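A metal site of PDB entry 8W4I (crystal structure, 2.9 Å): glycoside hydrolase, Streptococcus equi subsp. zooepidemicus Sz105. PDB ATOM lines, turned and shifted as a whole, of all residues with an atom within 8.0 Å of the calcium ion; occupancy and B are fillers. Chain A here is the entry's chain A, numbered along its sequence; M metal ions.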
ATOM      1  N   ASN A 760     -22.923  29.852  -7.606  1.00  0.00           N
ATOM      2  CA  ASN A 760     -23.663  29.575  -6.387  1.00  0.00           C
ATOM      3  C   ASN A 760     -24.489  28.306  -6.480  1.00  0.00           C
ATOM      4  O   ASN A 760     -24.711  27.633  -5.473  1.00  0.00           O
ATOM      5  CB  ASN A 760     -24.574  30.748  -6.052  1.00  0.00           C
ATOM      6  CG  ASN A 760     -23.963  31.685  -5.075  1.00  0.00           C
ATOM      7  OD1 ASN A 760     -23.070  31.304  -4.335  1.00  0.00           O
ATOM      8  ND2 ASN A 760     -24.456  32.920  -5.027  1.00  0.00           N
ATOM      9  N   ALA A 761     -24.952  27.974  -7.686  1.00  0.00           N
ATOM     10  CA  ALA A 761     -25.721  26.753  -7.874  1.00  0.00           C
ATOM     11  C   ALA A 761     -24.874  25.510  -7.657  1.00  0.00           C
ATOM     12  O   ALA A 761     -25.382  24.497  -7.165  1.00  0.00           O
ATOM     13  CB  ALA A 761     -26.352  26.733  -9.270  1.00  0.00           C
ATOM     14  N   LYS A 762     -23.587  25.553  -8.034  1.00  0.00           N
ATOM     15  CA  LYS A 762     -22.789  24.338  -7.867  1.00  0.00           C
ATOM     16  C   LYS A 762     -22.627  24.008  -6.388  1.00  0.00           C
ATOM     17  O   LYS A 762     -22.354  22.853  -6.044  1.00  0.00           O
ATOM     18  CB  LYS A 762     -21.403  24.460  -8.504  1.00  0.00           C
ATOM     19  CG  LYS A 762     -20.689  23.093  -8.572  1.00  0.00           C
ATOM     20  CD  LYS A 762     -19.197  23.159  -8.849  1.00  0.00           C
ATOM     21  CE  LYS A 762     -18.725  23.514 -10.251  1.00  0.00           C
ATOM     22  NZ  LYS A 762     -17.233  23.390 -10.166  1.00  0.00           N
ATOM     23  N   LYS A 763     -22.793  24.987  -5.500  1.00  0.00           N
ATOM     24  CA  LYS A 763     -22.781  24.763  -4.065  1.00  0.00           C
ATOM     25  C   LYS A 763     -24.070  24.126  -3.548  1.00  0.00           C
ATOM     26  O   LYS A 763     -24.121  23.759  -2.367  1.00  0.00           O
ATOM     27  CB  LYS A 763     -22.563  26.064  -3.283  1.00  0.00           C
ATOM     28  CG  LYS A 763     -21.567  27.048  -3.857  1.00  0.00           C
ATOM     29  CD  LYS A 763     -21.630  28.330  -3.056  1.00  0.00           C
ATOM     30  CE  LYS A 763     -20.666  29.379  -3.561  1.00  0.00           C
ATOM     31  NZ  LYS A 763     -20.944  30.710  -2.947  1.00  0.00           N
ATOM     32  N   VAL A 764     -25.110  24.026  -4.373  1.00  0.00           N
ATOM     33  CA  VAL A 764     -26.296  23.280  -3.966  1.00  0.00           C
ATOM     34  C   VAL A 764     -26.021  21.791  -3.925  1.00  0.00           C
ATOM     35  O   VAL A 764     -26.811  21.026  -3.360  1.00  0.00           O
ATOM     36  CB  VAL A 764     -27.465  23.621  -4.908  1.00  0.00           C
ATOM     37  CG1 VAL A 764     -28.761  22.977  -4.441  1.00  0.00           C
ATOM     38  CG2 VAL A 764     -27.647  25.133  -5.003  1.00  0.00           C
ATOM     39  N   PHE A 765     -24.878  21.360  -4.464  1.00  0.00           N
ATOM     40  CA  PHE A 765     -24.524  19.945  -4.517  1.00  0.00           C
ATOM     41  C   PHE A 765     -23.105  19.678  -3.998  1.00  0.00           C
ATOM     42  O   PHE A 765     -22.526  18.642  -4.320  1.00  0.00           O
ATOM     43  CB  PHE A 765     -24.684  19.409  -5.932  1.00  0.00           C
ATOM     44  CG  PHE A 765     -26.037  19.672  -6.525  1.00  0.00           C
ATOM     45  CD1 PHE A 765     -27.122  18.868  -6.188  1.00  0.00           C
ATOM     46  CD2 PHE A 765     -26.239  20.712  -7.421  1.00  0.00           C
ATOM     47  CE1 PHE A 765     -28.369  19.105  -6.729  1.00  0.00           C
ATOM     48  CE2 PHE A 765     -27.487  20.949  -7.961  1.00  0.00           C
ATOM     49  CZ  PHE A 765     -28.553  20.152  -7.610  1.00  0.00           C
ATOM     50  N   ASP A 766     -22.556  20.592  -3.200  1.00  0.00           N
ATOM     51  CA  ASP A 766     -21.196  20.440  -2.691  1.00  0.00           C
ATOM     52  C   ASP A 766     -21.142  19.630  -1.396  1.00  0.00           C
ATOM     53  O   ASP A 766     -20.124  19.682  -0.696  1.00  0.00           O
ATOM     54  CB  ASP A 766     -20.537  21.805  -2.499  1.00  0.00           C
ATOM     55  CG  ASP A 766     -21.263  22.677  -1.475  1.00  0.00           C
ATOM     56  OD1 ASP A 766     -22.319  22.262  -0.954  1.00  0.00           O
ATOM     57  OD2 ASP A 766     -20.764  23.793  -1.191  1.00  0.00           O
ATOM     58  N   GLY A 767     -22.207  18.905  -1.061  1.00  0.00           N
ATOM     59  CA  GLY A 767     -22.203  18.058   0.117  1.00  0.00           C
ATOM     60  C   GLY A 767     -21.979  18.819   1.411  1.00  0.00           C
ATOM     61  O   GLY A 767     -21.298  18.315   2.313  1.00  0.00           O
ATOM     62  N   LEU A 768     -22.556  20.020   1.521  1.00  0.00           N
ATOM     63  CA  LEU A 768     -22.377  20.879   2.685  1.00  0.00           C
ATOM     64  C   LEU A 768     -23.672  21.646   2.901  1.00  0.00           C
ATOM     65  O   LEU A 768     -24.177  22.279   1.975  1.00  0.00           O
ATOM     66  CB  LEU A 768     -21.196  21.843   2.464  1.00  0.00           C
ATOM     67  CG  LEU A 768     -20.691  22.652   3.663  1.00  0.00           C
ATOM     68  CD1 LEU A 768     -19.233  23.038   3.489  1.00  0.00           C
ATOM     69  CD2 LEU A 768     -21.527  23.887   3.949  1.00  0.00           C
ATOM     70  N   LEU A 769     -24.188  21.617   4.135  1.00  0.00           N
ATOM     71  CA  LEU A 769     -25.474  22.235   4.432  1.00  0.00           C
ATOM     72  C   LEU A 769     -25.325  23.704   4.835  1.00  0.00           C
ATOM     73  O   LEU A 769     -25.929  24.580   4.228  1.00  0.00           O
ATOM     74  CB  LEU A 769     -26.183  21.481   5.560  1.00  0.00           C
ATOM     75  CG  LEU A 769     -26.427  19.981   5.402  1.00  0.00           C
ATOM     76  CD1 LEU A 769     -27.389  19.483   6.466  1.00  0.00           C
ATOM     77  CD2 LEU A 769     -26.937  19.656   4.031  1.00  0.00           C
ATOM     78  N   ASN A 770     -24.525  23.967   5.873  1.00  0.00           N
ATOM     79  CA  ASN A 770     -24.380  25.323   6.412  1.00  0.00           C
ATOM     80  C   ASN A 770     -23.392  26.121   5.570  1.00  0.00           C
ATOM     81  O   ASN A 770     -22.354  26.595   6.041  1.00  0.00           O
ATOM     82  CB  ASN A 770     -23.964  25.257   7.873  1.00  0.00           C
ATOM     83  CG  ASN A 770     -25.086  24.784   8.777  1.00  0.00           C
ATOM     84  OD1 ASN A 770     -25.866  25.582   9.298  1.00  0.00           O
ATOM     85  ND2 ASN A 770     -25.190  23.470   8.960  1.00  0.00           N
ATOM     86  N   ASN A 771     -23.736  26.283   4.299  1.00  0.00           N
ATOM     87  CA  ASN A 771     -22.909  27.031   3.355  1.00  0.00           C
ATOM     88  C   ASN A 771     -22.977  28.505   3.732  1.00  0.00           C
ATOM     89  O   ASN A 771     -23.882  29.224   3.298  1.00  0.00           O
ATOM     90  CB  ASN A 771     -23.366  26.805   1.918  1.00  0.00           C
ATOM     91  CG  ASN A 771     -22.677  25.634   1.243  1.00  0.00           C
ATOM     92  OD1 ASN A 771     -21.448  25.555   1.209  1.00  0.00           O
ATOM     93  ND2 ASN A 771     -23.463  24.719   0.701  1.00  0.00           N
ATOM     94  N   THR A 773     -20.686  30.185   2.624  1.00  0.00           N
ATOM     95  CA  THR A 773     -20.063  30.650   1.398  1.00  0.00           C
ATOM     96  C   THR A 773     -21.099  31.254   0.446  1.00  0.00           C
ATOM     97  O   THR A 773     -20.860  31.273  -0.771  1.00  0.00           O
ATOM     98  CB  THR A 773     -19.295  29.515   0.716  1.00  0.00           C
ATOM     99  OG1 THR A 773     -18.666  29.996  -0.471  1.00  0.00           O
ATOM    100  CG2 THR A 773     -20.213  28.361   0.382  1.00  0.00           C
ATOM    101  N   THR A 775     -24.955  30.781  -0.367  1.00  0.00           N
ATOM    102  CA  THR A 775     -25.618  29.771  -1.195  1.00  0.00           C
ATOM    103  C   THR A 775     -26.894  30.284  -1.862  1.00  0.00           C
ATOM    104  O   THR A 775     -27.913  29.593  -1.903  1.00  0.00           O
ATOM    105  CB  THR A 775     -25.914  28.534  -0.366  1.00  0.00           C
ATOM    106  OG1 THR A 775     -26.656  27.602  -1.153  1.00  0.00           O
ATOM    107  CG2 THR A 775     -26.721  28.908   0.891  1.00  0.00           C
ATOM    108  N   PHE A 800     -32.712  21.804   1.993  1.00  0.00           N
ATOM    109  CA  PHE A 800     -32.528  22.584   3.204  1.00  0.00           C
ATOM    110  C   PHE A 800     -32.675  24.065   2.890  1.00  0.00           C
ATOM    111  O   PHE A 800     -32.414  24.500   1.762  1.00  0.00           O
ATOM    112  CB  PHE A 800     -31.145  22.317   3.829  1.00  0.00           C
ATOM    113  CG  PHE A 800     -30.868  20.867   4.088  1.00  0.00           C
ATOM    114  CD1 PHE A 800     -30.440  20.031   3.063  1.00  0.00           C
ATOM    115  CD2 PHE A 800     -31.042  20.322   5.354  1.00  0.00           C
ATOM    116  CE1 PHE A 800     -30.195  18.694   3.292  1.00  0.00           C
ATOM    117  CE2 PHE A 800     -30.785  18.982   5.591  1.00  0.00           C
ATOM    118  CZ  PHE A 800     -30.363  18.168   4.555  1.00  0.00           C
ATOM    119  N   LEU A 880     -30.699  28.455  -1.792  1.00  0.00           N
ATOM    120  CA  LEU A 880     -30.818  27.002  -1.699  1.00  0.00           C
ATOM    121  C   LEU A 880     -29.483  26.421  -1.236  1.00  0.00           C
ATOM    122  O   LEU A 880     -28.583  26.212  -2.060  1.00  0.00           O
ATOM    123  CB  LEU A 880     -31.250  26.390  -3.032  1.00  0.00           C
ATOM    124  CG  LEU A 880     -31.467  24.873  -2.998  1.00  0.00           C
ATOM    125  CD1 LEU A 880     -32.345  24.475  -1.820  1.00  0.00           C
ATOM    126  CD2 LEU A 880     -32.067  24.387  -4.306  1.00  0.00           C
ATOM    127  N   PRO A 881     -29.336  26.159   0.064  1.00  0.00           N
ATOM    128  CA  PRO A 881     -28.054  25.599   0.543  1.00  0.00           C
ATOM    129  C   PRO A 881     -27.678  24.275  -0.083  1.00  0.00           C
ATOM    130  O   PRO A 881     -26.573  24.146  -0.621  1.00  0.00           O
ATOM    131  CB  PRO A 881     -28.299  25.455   2.056  1.00  0.00           C
ATOM    132  CG  PRO A 881     -29.274  26.470   2.349  1.00  0.00           C
ATOM    133  CD  PRO A 881     -30.195  26.567   1.176  1.00  0.00           C
ATOM    134  N   GLU A 882     -28.573  23.299  -0.047  1.00  0.00           N
ATOM    135  CA  GLU A 882     -28.193  21.920  -0.322  1.00  0.00           C
ATOM    136  C   GLU A 882     -29.422  21.136  -0.731  1.00  0.00           C
ATOM    137  O   GLU A 882     -30.391  21.060   0.052  1.00  0.00           O
ATOM    138  CB  GLU A 882     -27.542  21.292   0.904  1.00  0.00           C
ATOM    139  CG  GLU A 882     -27.111  19.834   0.755  1.00  0.00           C
ATOM    140  CD  GLU A 882     -25.976  19.603  -0.228  1.00  0.00           C
ATOM    141  OE1 GLU A 882     -25.470  20.562  -0.842  1.00  0.00           O
ATOM    142  OE2 GLU A 882     -25.540  18.431  -0.325  1.00  0.00           O
ATOM    143  N   LEU A 883     -29.402  20.548  -1.917  1.00  0.00           N
ATOM    144  CA  LEU A 883     -30.449  19.655  -2.355  1.00  0.00           C
ATOM    145  C   LEU A 883     -29.873  18.272  -2.640  1.00  0.00           C
ATOM    146  O   LEU A 883     -28.816  18.134  -3.257  1.00  0.00           O
ATOM    147  CB  LEU A 883     -31.167  20.220  -3.575  1.00  0.00           C
ATOM    148  CG  LEU A 883     -32.332  19.399  -4.128  1.00  0.00           C
ATOM    149  CD1 LEU A 883     -33.400  20.302  -4.681  1.00  0.00           C
ATOM    150  CD2 LEU A 883     -31.759  18.599  -5.277  1.00  0.00           C
HETATM  151 CA    CA M   1     -24.660  22.750  -0.326  1.00  0.00          CA
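O of Pro 881 lies close to OG1 of Thr 775 (3.5 Å).
The backbone NH of Phe 800 lies within hydrogen-bond range of the backbone carbonyl oxygen of Glu 882, 3.1 Å away.
The side-chain amino group (NZ) of Lys 763 lies within hydrogen-bond range of the side-chain amide oxygen (OD1) of Asn 760, 2.6 Å away.
The backbone carbonyl oxygen (O) of Val 764 is in hydrogen-bond range of the backbone NH (N) of Leu 883 (3.0 Å).
NZ of Lys 763 is in hydrogen-bond range of OG1 of Thr 773 (3.4 Å).
The backbone NH (N) of Gly 767 lies close to the side-chain carboxylate (OE2) of Glu 882 (3.4 Å).
C of Val 764 touches the calcium ion (3.97 Å).
Seven residues have an atom within 4 Å of the calcium ion: Lys 763, Val 764, Asp 766, Leu 768, Asn 771, Pro 881 and Glu 882.
The nearest printed residue that does not touch the calcium ion is Phe 765 (4.4 Å).
The calcium ion is bound by the backbone carbonyl oxygen of Lys 763 (2.3 Å), the backbone carbonyl oxygen of Pro 881 (2.4 Å), the side-chain carboxylate of Glu 882 (2.4 Å), the backbone carbonyl oxygen of Leu 768 (2.4 Å), the side-chain carboxylate of Asp 766 (2.5 Å) and the side-chain amide nitrogen of Asn 771 (2.5 Å).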
